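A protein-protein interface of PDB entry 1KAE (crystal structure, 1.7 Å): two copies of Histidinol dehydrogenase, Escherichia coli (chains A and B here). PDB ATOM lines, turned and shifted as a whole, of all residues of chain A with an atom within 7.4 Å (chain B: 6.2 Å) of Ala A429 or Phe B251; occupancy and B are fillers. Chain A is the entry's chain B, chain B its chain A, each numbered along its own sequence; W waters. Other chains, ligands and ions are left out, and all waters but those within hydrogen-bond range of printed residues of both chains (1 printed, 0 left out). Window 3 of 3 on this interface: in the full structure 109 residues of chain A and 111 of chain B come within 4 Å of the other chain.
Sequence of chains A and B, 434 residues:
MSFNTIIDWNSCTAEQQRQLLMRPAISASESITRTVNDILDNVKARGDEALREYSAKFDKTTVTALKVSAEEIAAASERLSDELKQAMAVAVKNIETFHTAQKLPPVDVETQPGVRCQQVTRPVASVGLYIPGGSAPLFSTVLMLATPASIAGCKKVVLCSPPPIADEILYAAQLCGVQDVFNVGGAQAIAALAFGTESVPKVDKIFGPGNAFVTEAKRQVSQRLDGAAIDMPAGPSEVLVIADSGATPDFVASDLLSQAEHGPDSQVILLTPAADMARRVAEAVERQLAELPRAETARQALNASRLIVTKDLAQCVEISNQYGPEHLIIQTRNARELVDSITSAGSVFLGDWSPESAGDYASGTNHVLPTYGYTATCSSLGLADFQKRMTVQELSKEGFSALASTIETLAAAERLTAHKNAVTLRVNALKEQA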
ATOM      1  N   ASN A 421     -20.347   3.240 -18.452  1.00  0.00           N
ATOM      2  CA  ASN A 421     -21.794   3.542 -18.344  1.00  0.00           C
ATOM      3  C   ASN A 421     -22.218   4.885 -18.914  1.00  0.00           C
ATOM      4  O   ASN A 421     -23.349   5.023 -19.428  1.00  0.00           O
ATOM      5  CB  ASN A 421     -22.238   3.433 -16.894  1.00  0.00           C
ATOM      6  CG  ASN A 421     -22.284   1.995 -16.422  1.00  0.00           C
ATOM      7  OD1 ASN A 421     -22.051   1.074 -17.200  1.00  0.00           O
ATOM      8  ND2 ASN A 421     -22.584   1.790 -15.142  1.00  0.00           N
ATOM      9  N   ALA A 422     -21.325   5.882 -18.881  1.00  0.00           N
ATOM     10  CA  ALA A 422     -21.687   7.202 -19.417  1.00  0.00           C
ATOM     11  C   ALA A 422     -21.861   7.055 -20.924  1.00  0.00           C
ATOM     12  O   ALA A 422     -22.636   7.816 -21.545  1.00  0.00           O
ATOM     13  CB  ALA A 422     -20.597   8.261 -19.089  1.00  0.00           C
ATOM     14  N   VAL A 423     -21.176   6.071 -21.507  1.00  0.00           N
ATOM     15  CA  VAL A 423     -21.311   5.838 -22.949  1.00  0.00           C
ATOM     16  C   VAL A 423     -22.554   5.011 -23.204  1.00  0.00           C
ATOM     17  O   VAL A 423     -23.393   5.376 -24.041  1.00  0.00           O
ATOM     18  CB  VAL A 423     -20.067   5.152 -23.499  1.00  0.00           C
ATOM     19  CG1 VAL A 423     -20.265   4.772 -25.037  1.00  0.00           C
ATOM     20  CG2 VAL A 423     -18.844   6.101 -23.244  1.00  0.00           C
ATOM     21  N   THR A 424     -22.734   3.931 -22.462  1.00  0.00           N
ATOM     22  CA  THR A 424     -23.925   3.070 -22.647  1.00  0.00           C
ATOM     23  C   THR A 424     -25.267   3.821 -22.557  1.00  0.00           C
ATOM     24  O   THR A 424     -26.161   3.604 -23.392  1.00  0.00           O
ATOM     25  CB  THR A 424     -23.909   1.920 -21.650  1.00  0.00           C
ATOM     26  OG1 THR A 424     -22.754   1.091 -21.909  1.00  0.00           O
ATOM     27  CG2 THR A 424     -25.184   1.020 -21.850  1.00  0.00           C
ATOM     28  N   LEU A 425     -25.422   4.678 -21.545  1.00  0.00           N
ATOM     29  CA  LEU A 425     -26.628   5.491 -21.358  1.00  0.00           C
ATOM     30  C   LEU A 425     -26.965   6.292 -22.620  1.00  0.00           C
ATOM     31  O   LEU A 425     -28.138   6.364 -23.004  1.00  0.00           O
ATOM     32  CB  LEU A 425     -26.473   6.478 -20.187  1.00  0.00           C
ATOM     33  CG  LEU A 425     -26.644   5.801 -18.836  1.00  0.00           C
ATOM     34  CD1 LEU A 425     -26.092   6.679 -17.755  1.00  0.00           C
ATOM     35  CD2 LEU A 425     -28.137   5.482 -18.646  1.00  0.00           C
ATOM     36  N   ARG A 426     -25.961   6.899 -23.244  1.00  0.00           N
ATOM     37  CA  ARG A 426     -26.199   7.670 -24.456  1.00  0.00           C
ATOM     38  C   ARG A 426     -26.533   6.780 -25.656  1.00  0.00           C
ATOM     39  O   ARG A 426     -27.416   7.120 -26.449  1.00  0.00           O
ATOM     40  CB  ARG A 426     -24.983   8.565 -24.723  1.00  0.00           C
ATOM     41  CG  ARG A 426     -24.860   9.692 -23.623  1.00  0.00           C
ATOM     42  CD  ARG A 426     -23.424  10.177 -23.537  1.00  0.00           C
ATOM     43  NE  ARG A 426     -23.300  11.502 -22.925  1.00  0.00           N
ATOM     44  CZ  ARG A 426     -23.079  11.739 -21.636  1.00  0.00           C
ATOM     45  NH1 ARG A 426     -22.968  10.734 -20.757  1.00  0.00           N
ATOM     46  NH2 ARG A 426     -22.916  12.987 -21.247  1.00  0.00           N
ATOM     47  N   VAL A 427     -25.852   5.643 -25.795  1.00  0.00           N
ATOM     48  CA  VAL A 427     -26.118   4.716 -26.910  1.00  0.00           C
ATOM     49  C   VAL A 427     -27.583   4.277 -26.796  1.00  0.00           C
ATOM     50  O   VAL A 427     -28.339   4.286 -27.806  1.00  0.00           O
ATOM     51  CB  VAL A 427     -25.200   3.458 -26.824  1.00  0.00           C
ATOM     52  CG1 VAL A 427     -25.693   2.361 -27.803  1.00  0.00           C
ATOM     53  CG2 VAL A 427     -23.759   3.838 -27.167  1.00  0.00           C
ATOM     54  N   ASN A 428     -28.013   3.943 -25.576  1.00  0.00           N
ATOM     55  CA  ASN A 428     -29.408   3.517 -25.392  1.00  0.00           C
ATOM     56  C   ASN A 428     -30.425   4.630 -25.665  1.00  0.00           C
ATOM     57  O   ASN A 428     -31.435   4.380 -26.334  1.00  0.00           O
ATOM     58  CB  ASN A 428     -29.618   2.898 -24.003  1.00  0.00           C
ATOM     59  CG  ASN A 428     -28.929   1.557 -23.869  1.00  0.00           C
ATOM     60  OD1 ASN A 428     -28.710   0.870 -24.864  1.00  0.00           O
ATOM     61  ND2 ASN A 428     -28.605   1.159 -22.649  1.00  0.00           N
ATOM     62  N   ALA A 429     -30.157   5.859 -25.202  1.00  0.00           N
ATOM     63  CA  ALA A 429     -31.072   6.973 -25.452  1.00  0.00           C
ATOM     64  C   ALA A 429     -31.186   7.230 -26.963  1.00  0.00           C
ATOM     65  O   ALA A 429     -32.273   7.591 -27.458  1.00  0.00           O
ATOM     66  CB  ALA A 429     -30.589   8.230 -24.725  1.00  0.00           C
ATOM     67  N   LEU A 430     -30.094   7.058 -27.706  1.00  0.00           N
ATOM     68  CA  LEU A 430     -30.130   7.270 -29.160  1.00  0.00           C
ATOM     69  C   LEU A 430     -30.908   6.163 -29.893  1.00  0.00           C
ATOM     70  O   LEU A 430     -31.613   6.449 -30.861  1.00  0.00           O
ATOM     71  CB  LEU A 430     -28.713   7.390 -29.744  1.00  0.00           C
ATOM     72  CG  LEU A 430     -28.035   8.729 -29.392  1.00  0.00           C
ATOM     73  CD1 LEU A 430     -26.549   8.661 -29.713  1.00  0.00           C
ATOM     74  CD2 LEU A 430     -28.703   9.909 -30.147  1.00  0.00           C
ATOM     75  N   LYS A 431     -30.745   4.910 -29.469  1.00  0.00           N
ATOM     76  CA  LYS A 431     -31.494   3.802 -30.071  1.00  0.00           C
ATOM     77  C   LYS A 431     -32.968   4.067 -29.791  1.00  0.00           C
ATOM     78  O   LYS A 431     -33.798   3.932 -30.679  1.00  0.00           O
ATOM     79  CB  LYS A 431     -31.149   2.460 -29.424  1.00  0.00           C
ATOM     80  CG  LYS A 431     -29.786   1.904 -29.760  1.00  0.00           C
ATOM     81  CD  LYS A 431     -29.571   0.531 -29.125  1.00  0.00           C
ATOM     82  CE  LYS A 431     -29.827   0.598 -27.621  1.00  0.00           C
ATOM     83  NZ  LYS A 431     -29.605  -0.715 -27.029  1.00  0.00           N
ATOM     84  N   GLU A 432     -33.282   4.426 -28.545  1.00  0.00           N
ATOM     85  CA  GLU A 432     -34.651   4.708 -28.105  1.00  0.00           C
ATOM     86  C   GLU A 432     -35.387   5.731 -28.967  1.00  0.00           C
ATOM     87  O   GLU A 432     -36.611   5.660 -29.120  1.00  0.00           O
ATOM     88  CB  GLU A 432     -34.651   5.240 -26.675  1.00  0.00           C
ATOM     89  CG  GLU A 432     -34.210   4.255 -25.616  1.00  0.00           C
ATOM     90  CD  GLU A 432     -35.359   3.451 -25.085  1.00  0.00           C
ATOM     91  OE1 GLU A 432     -36.438   4.051 -24.844  1.00  0.00           O
ATOM     92  OE2 GLU A 432     -35.185   2.231 -24.897  1.00  0.00           O
ATOM     93  N   GLN A 433     -34.652   6.699 -29.502  1.00  0.00           N
ATOM     94  CA  GLN A 433     -35.264   7.736 -30.327  1.00  0.00           C
ATOM     95  C   GLN A 433     -35.122   7.355 -31.789  1.00  0.00           C
ATOM     96  O   GLN A 433     -35.806   7.910 -32.657  1.00  0.00           O
ATOM     97  CB  GLN A 433     -34.588   9.095 -30.073  1.00  0.00           C
ATOM     98  CG  GLN A 433     -33.098   9.112 -30.383  1.00  0.00           C
ATOM     99  CD  GLN A 433     -32.496  10.518 -30.455  1.00  0.00           C
ATOM    100  OE1 GLN A 433     -32.565  11.291 -29.493  1.00  0.00           O
ATOM    101  NE2 GLN A 433     -31.889  10.845 -31.600  1.00  0.00           N
ATOM    102  N   ALA A 434     -34.250   6.384 -32.051  1.00  0.00           N
ATOM    103  CA  ALA A 434     -33.967   5.928 -33.404  1.00  0.00           C
ATOM    104  C   ALA A 434     -33.567   4.458 -33.460  1.00  0.00           C
ATOM    105  O   ALA A 434     -32.352   4.186 -33.653  1.00  0.00           O
ATOM    106  CB  ALA A 434     -32.856   6.781 -34.016  1.00  0.00           C
ATOM    107  OXT ALA A 434     -34.470   3.603 -33.311  1.00  0.00           O
ATOM    108  N   THR B 248     -30.170  16.159 -19.724  1.00  0.00           N
ATOM    109  CA  THR B 248     -30.744  14.868 -19.351  1.00  0.00           C
ATOM    110  C   THR B 248     -30.072  14.479 -18.018  1.00  0.00           C
ATOM    111  O   THR B 248     -28.861  14.232 -17.985  1.00  0.00           O
ATOM    112  CB  THR B 248     -30.418  13.860 -20.435  1.00  0.00           C
ATOM    113  OG1 THR B 248     -31.119  14.254 -21.637  1.00  0.00           O
ATOM    114  CG2 THR B 248     -30.804  12.441 -20.000  1.00  0.00           C
ATOM    115  N   PRO B 249     -30.851  14.411 -16.907  1.00  0.00           N
ATOM    116  CA  PRO B 249     -30.250  14.073 -15.610  1.00  0.00           C
ATOM    117  C   PRO B 249     -29.366  12.848 -15.621  1.00  0.00           C
ATOM    118  O   PRO B 249     -28.283  12.861 -15.030  1.00  0.00           O
ATOM    119  CB  PRO B 249     -31.458  13.932 -14.695  1.00  0.00           C
ATOM    120  CG  PRO B 249     -32.394  14.988 -15.280  1.00  0.00           C
ATOM    121  CD  PRO B 249     -32.275  14.719 -16.758  1.00  0.00           C
ATOM    122  N   ASP B 250     -29.805  11.786 -16.292  1.00  0.00           N
ATOM    123  CA  ASP B 250     -28.988  10.601 -16.301  1.00  0.00           C
ATOM    124  C   ASP B 250     -27.639  10.827 -16.973  1.00  0.00           C
ATOM    125  O   ASP B 250     -26.654  10.223 -16.571  1.00  0.00           O
ATOM    126  CB  ASP B 250     -29.733   9.446 -16.962  1.00  0.00           C
ATOM    127  CG  ASP B 250     -30.771   8.838 -16.042  1.00  0.00           C
ATOM    128  OD1 ASP B 250     -30.485   8.656 -14.845  1.00  0.00           O
ATOM    129  OD2 ASP B 250     -31.876   8.535 -16.512  1.00  0.00           O
ATOM    130  N   PHE B 251     -27.566  11.671 -17.998  1.00  0.00           N
ATOM    131  CA  PHE B 251     -26.277  11.901 -18.661  1.00  0.00           C
ATOM    132  C   PHE B 251     -25.362  12.664 -17.714  1.00  0.00           C
ATOM    133  O   PHE B 251     -24.156  12.336 -17.584  1.00  0.00           O
ATOM    134  CB  PHE B 251     -26.447  12.750 -19.936  1.00  0.00           C
ATOM    135  CG  PHE B 251     -27.170  12.049 -21.075  1.00  0.00           C
ATOM    136  CD1 PHE B 251     -27.695  10.771 -20.927  1.00  0.00           C
ATOM    137  CD2 PHE B 251     -27.337  12.703 -22.296  1.00  0.00           C
ATOM    138  CE1 PHE B 251     -28.393  10.122 -21.995  1.00  0.00           C
ATOM    139  CE2 PHE B 251     -28.020  12.100 -23.349  1.00  0.00           C
ATOM    140  CZ  PHE B 251     -28.552  10.805 -23.209  1.00  0.00           C
ATOM    141  N   VAL B 252     -25.915  13.681 -17.049  1.00  0.00           N
ATOM    142  CA  VAL B 252     -25.137  14.514 -16.114  1.00  0.00           C
ATOM    143  C   VAL B 252     -24.548  13.634 -15.000  1.00  0.00           C
ATOM    144  O   VAL B 252     -23.321  13.688 -14.697  1.00  0.00           O
ATOM    145  CB  VAL B 252     -26.074  15.630 -15.512  1.00  0.00           C
ATOM    146  CG1 VAL B 252     -25.388  16.394 -14.367  1.00  0.00           C
ATOM    147  CG2 VAL B 252     -26.472  16.642 -16.616  1.00  0.00           C
ATOM    148  N   ALA B 253     -25.430  12.829 -14.403  1.00  0.00           N
ATOM    149  CA  ALA B 253     -25.068  11.948 -13.307  1.00  0.00           C
ATOM    150  C   ALA B 253     -23.972  10.970 -13.699  1.00  0.00           C
ATOM    151  O   ALA B 253     -23.050  10.683 -12.916  1.00  0.00           O
ATOM    152  CB  ALA B 253     -26.310  11.160 -12.849  1.00  0.00           C
ATOM    153  N   SER B 254     -24.077  10.423 -14.907  1.00  0.00           N
ATOM    154  CA  SER B 254     -23.100   9.455 -15.351  1.00  0.00           C
ATOM    155  C   SER B 254     -21.743  10.097 -15.552  1.00  0.00           C
ATOM    156  O   SER B 254     -20.694   9.432 -15.350  1.00  0.00           O
ATOM    157  CB  SER B 254     -23.588   8.745 -16.623  1.00  0.00           C
ATOM    158  OG  SER B 254     -23.559   9.584 -17.781  1.00  0.00           O
ATOM    159  N   ASP B 255     -21.723  11.375 -15.973  1.00  0.00           N
ATOM    160  CA  ASP B 255     -20.449  12.053 -16.172  1.00  0.00           C
ATOM    161  C   ASP B 255     -19.831  12.340 -14.792  1.00  0.00           C
ATOM    162  O   ASP B 255     -18.645  12.079 -14.581  1.00  0.00           O
ATOM    163  CB  ASP B 255     -20.611  13.354 -16.984  1.00  0.00           C
ATOM    164  CG  ASP B 255     -21.040  13.091 -18.438  1.00  0.00           C
ATOM    165  OD1 ASP B 255     -20.657  12.041 -19.007  1.00  0.00           O
ATOM    166  OD2 ASP B 255     -21.783  13.918 -19.017  1.00  0.00           O
ATOM    167  N   LEU B 256     -20.644  12.808 -13.844  1.00  0.00           N
ATOM    168  CA  LEU B 256     -20.144  13.082 -12.486  1.00  0.00           C
ATOM    169  C   LEU B 256     -19.572  11.769 -11.924  1.00  0.00           C
ATOM    170  O   LEU B 256     -18.455  11.753 -11.397  1.00  0.00           O
ATOM    171  CB  LEU B 256     -21.279  13.589 -11.580  1.00  0.00           C
ATOM    172  CG  LEU B 256     -21.908  14.964 -11.923  1.00  0.00           C
ATOM    173  CD1 LEU B 256     -23.102  15.250 -11.002  1.00  0.00           C
ATOM    174  CD2 LEU B 256     -20.878  16.055 -11.752  1.00  0.00           C
ATOM    175  N   GLN B 288     -27.572   5.339  -9.927  1.00  0.00           N
ATOM    176  CA  GLN B 288     -26.496   4.831 -10.753  1.00  0.00           C
ATOM    177  C   GLN B 288     -25.324   4.360  -9.877  1.00  0.00           C
ATOM    178  O   GLN B 288     -24.649   3.368 -10.212  1.00  0.00           O
ATOM    179  CB  GLN B 288     -26.001   5.895 -11.739  1.00  0.00           C
ATOM    180  CG  GLN B 288     -26.950   6.139 -12.893  1.00  0.00           C
ATOM    181  CD  GLN B 288     -26.425   7.205 -13.857  1.00  0.00           C
ATOM    182  OE1 GLN B 288     -25.218   7.345 -14.068  1.00  0.00           O
ATOM    183  NE2 GLN B 288     -27.351   7.933 -14.482  1.00  0.00           N
ATOM    184  N   GLN B 331     -23.505  20.986 -20.779  1.00  0.00           N
ATOM    185  CA  GLN B 331     -24.705  20.339 -21.276  1.00  0.00           C
ATOM    186  C   GLN B 331     -25.803  21.352 -21.301  1.00  0.00           C
ATOM    187  O   GLN B 331     -26.717  21.319 -20.454  1.00  0.00           O
ATOM    188  CB  GLN B 331     -25.021  19.119 -20.395  1.00  0.00           C
ATOM    189  CG  GLN B 331     -23.964  17.977 -20.612  1.00  0.00           C
ATOM    190  CD  GLN B 331     -24.226  16.724 -19.813  1.00  0.00           C
ATOM    191  OE1 GLN B 331     -25.360  16.404 -19.506  1.00  0.00           O
ATOM    192  NE2 GLN B 331     -23.160  15.986 -19.487  1.00  0.00           N
ATOM    193  N   ASP B 352     -24.817  17.130 -25.365  1.00  0.00           N
ATOM    194  CA  ASP B 352     -25.171  15.860 -24.725  1.00  0.00           C
ATOM    195  C   ASP B 352     -24.439  14.617 -25.138  1.00  0.00           C
ATOM    196  O   ASP B 352     -24.500  13.620 -24.418  1.00  0.00           O
ATOM    197  CB  ASP B 352     -26.658  15.591 -24.914  1.00  0.00           C
ATOM    198  CG  ASP B 352     -27.525  16.623 -24.262  1.00  0.00           C
ATOM    199  OD1 ASP B 352     -27.097  17.302 -23.305  1.00  0.00           O
ATOM    200  OD2 ASP B 352     -28.676  16.760 -24.706  1.00  0.00           O
ATOM    201  N   TRP B 353     -23.745  14.651 -26.283  1.00  0.00           N
ATOM    202  CA  TRP B 353     -23.066  13.472 -26.823  1.00  0.00           C
ATOM    203  C   TRP B 353     -21.565  13.522 -26.651  1.00  0.00           C
ATOM    204  O   TRP B 353     -20.836  12.808 -27.323  1.00  0.00           O
ATOM    205  CB  TRP B 353     -23.436  13.277 -28.325  1.00  0.00           C
ATOM    206  CG  TRP B 353     -24.923  13.486 -28.493  1.00  0.00           C
ATOM    207  CD1 TRP B 353     -25.542  14.574 -29.045  1.00  0.00           C
ATOM    208  CD2 TRP B 353     -25.959  12.685 -27.917  1.00  0.00           C
ATOM    209  NE1 TRP B 353     -26.911  14.513 -28.831  1.00  0.00           N
ATOM    210  CE2 TRP B 353     -27.191  13.355 -28.144  1.00  0.00           C
ATOM    211  CE3 TRP B 353     -25.964  11.464 -27.219  1.00  0.00           C
ATOM    212  CZ2 TRP B 353     -28.432  12.845 -27.697  1.00  0.00           C
ATOM    213  CZ3 TRP B 353     -27.182  10.952 -26.764  1.00  0.00           C
ATOM    214  CH2 TRP B 353     -28.409  11.648 -27.005  1.00  0.00           C
HETATM  215  O   HOH W   1     -21.926  15.465 -22.713  1.00  0.00           O
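NE2 of Gln B331 sits close to NH2 of Arg A426 (3.5 Å).
NE of Arg A426 is in hydrogen-bond range of O of Asp B352 (2.9 Å).
OG of Ser B254 lies within hydrogen-bond range of NH1 of Arg A426 (3.2 Å).
The side-chain carboxylate of Asp B255 is in salt-bridge range of the guanidinium group of Arg A426 (2.7 Å).
The side-chain amide nitrogen (NE2) of Gln B331 is in hydrogen-bond range of the side-chain carboxylate (OD2) of Asp B255, at 2.5 Å.
The backbone NH of Ser B254 lies close to the side-chain amide oxygen of Gln B288.
The backbone carbonyl oxygen (O) of Asp B250 sits at hydrogen-bond distance from the side-chain hydroxyl (OG) of Ser B254 (3.4 Å).
The backbone carbonyl oxygen (O) of Ala A422 lies within hydrogen-bond range of the guanidinium group (NH1) of Arg A426 (3.0 Å).
The side-chain amide nitrogen (NE2) of Gln B288 lies within hydrogen-bond range of the backbone carbonyl oxygen (O) of Asp B250 (3.2 Å).
The backbone carbonyl oxygen of Phe B251 lies within hydrogen-bond range of the side-chain hydroxyl of Ser B254 (2.8 Å).
Among the printed residues, pairs that only touch across the chains: Ala A422 with Ser B254, Ala A422 with Asp B255, Leu A425 with Asp B250, Leu A425 with Phe B251, Leu A425 with Ser B254, Leu A425 with Gln B288, Arg A426 with Phe B251, Arg A426 with Trp B353, Ala A429 with Phe B251 and Leu A430 with Trp B353.
Printed residues of chain B within 4 Å of Ala A422: Ser B254 and Asp B255.
Ala A429 touches just one residue of chain B: Phe B251 (3.6 Å).
Of chain A, only Leu A425, Arg A426 and Ala A429 come within 4 Å of Phe B251.
Of the printed residues of chain A, Asp B255 touches Ala A422 (3.8 Å) and Arg A426 (2.7 Å).
Of the printed residues of chain A, Gln B331 touches Arg A426 (3.5 Å).
Of the printed residues of chain A, Asp B352 touches Arg A426 (2.9 Å).
The nearest residue of chain B that does not touch Ala A429 is Trp B353 (4.7 Å).
Hydrophobic or aromatic side chains of chain A that line the printed part of chain B: Ala A422, Leu A425, Ala A429 and Leu A430.
Of the 13 printed residues of chain B, 8 touch a printed residue of chain A.
Hydrophobic or aromatic side chains of chain B that line the printed part of chain A: Phe B251 and Trp B353.
Among the printed residues, 14 pairs touch across the chains.
Among the printed residues, Asp or Glu carboxylates within 4 Å of a Lys or Arg side-chain nitrogen of the other chain: Arg A426 with Asp B255 (2.7 Å).
No position is printed for both chains.
Of the 14 pairs that touch across the chains among the printed residues, none has its exchanged pair printed and touching as well.
Water W1 bridges NH2 of Arg A426 (3.0 Å) and NE2 of Gln B331 (3.5 Å).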
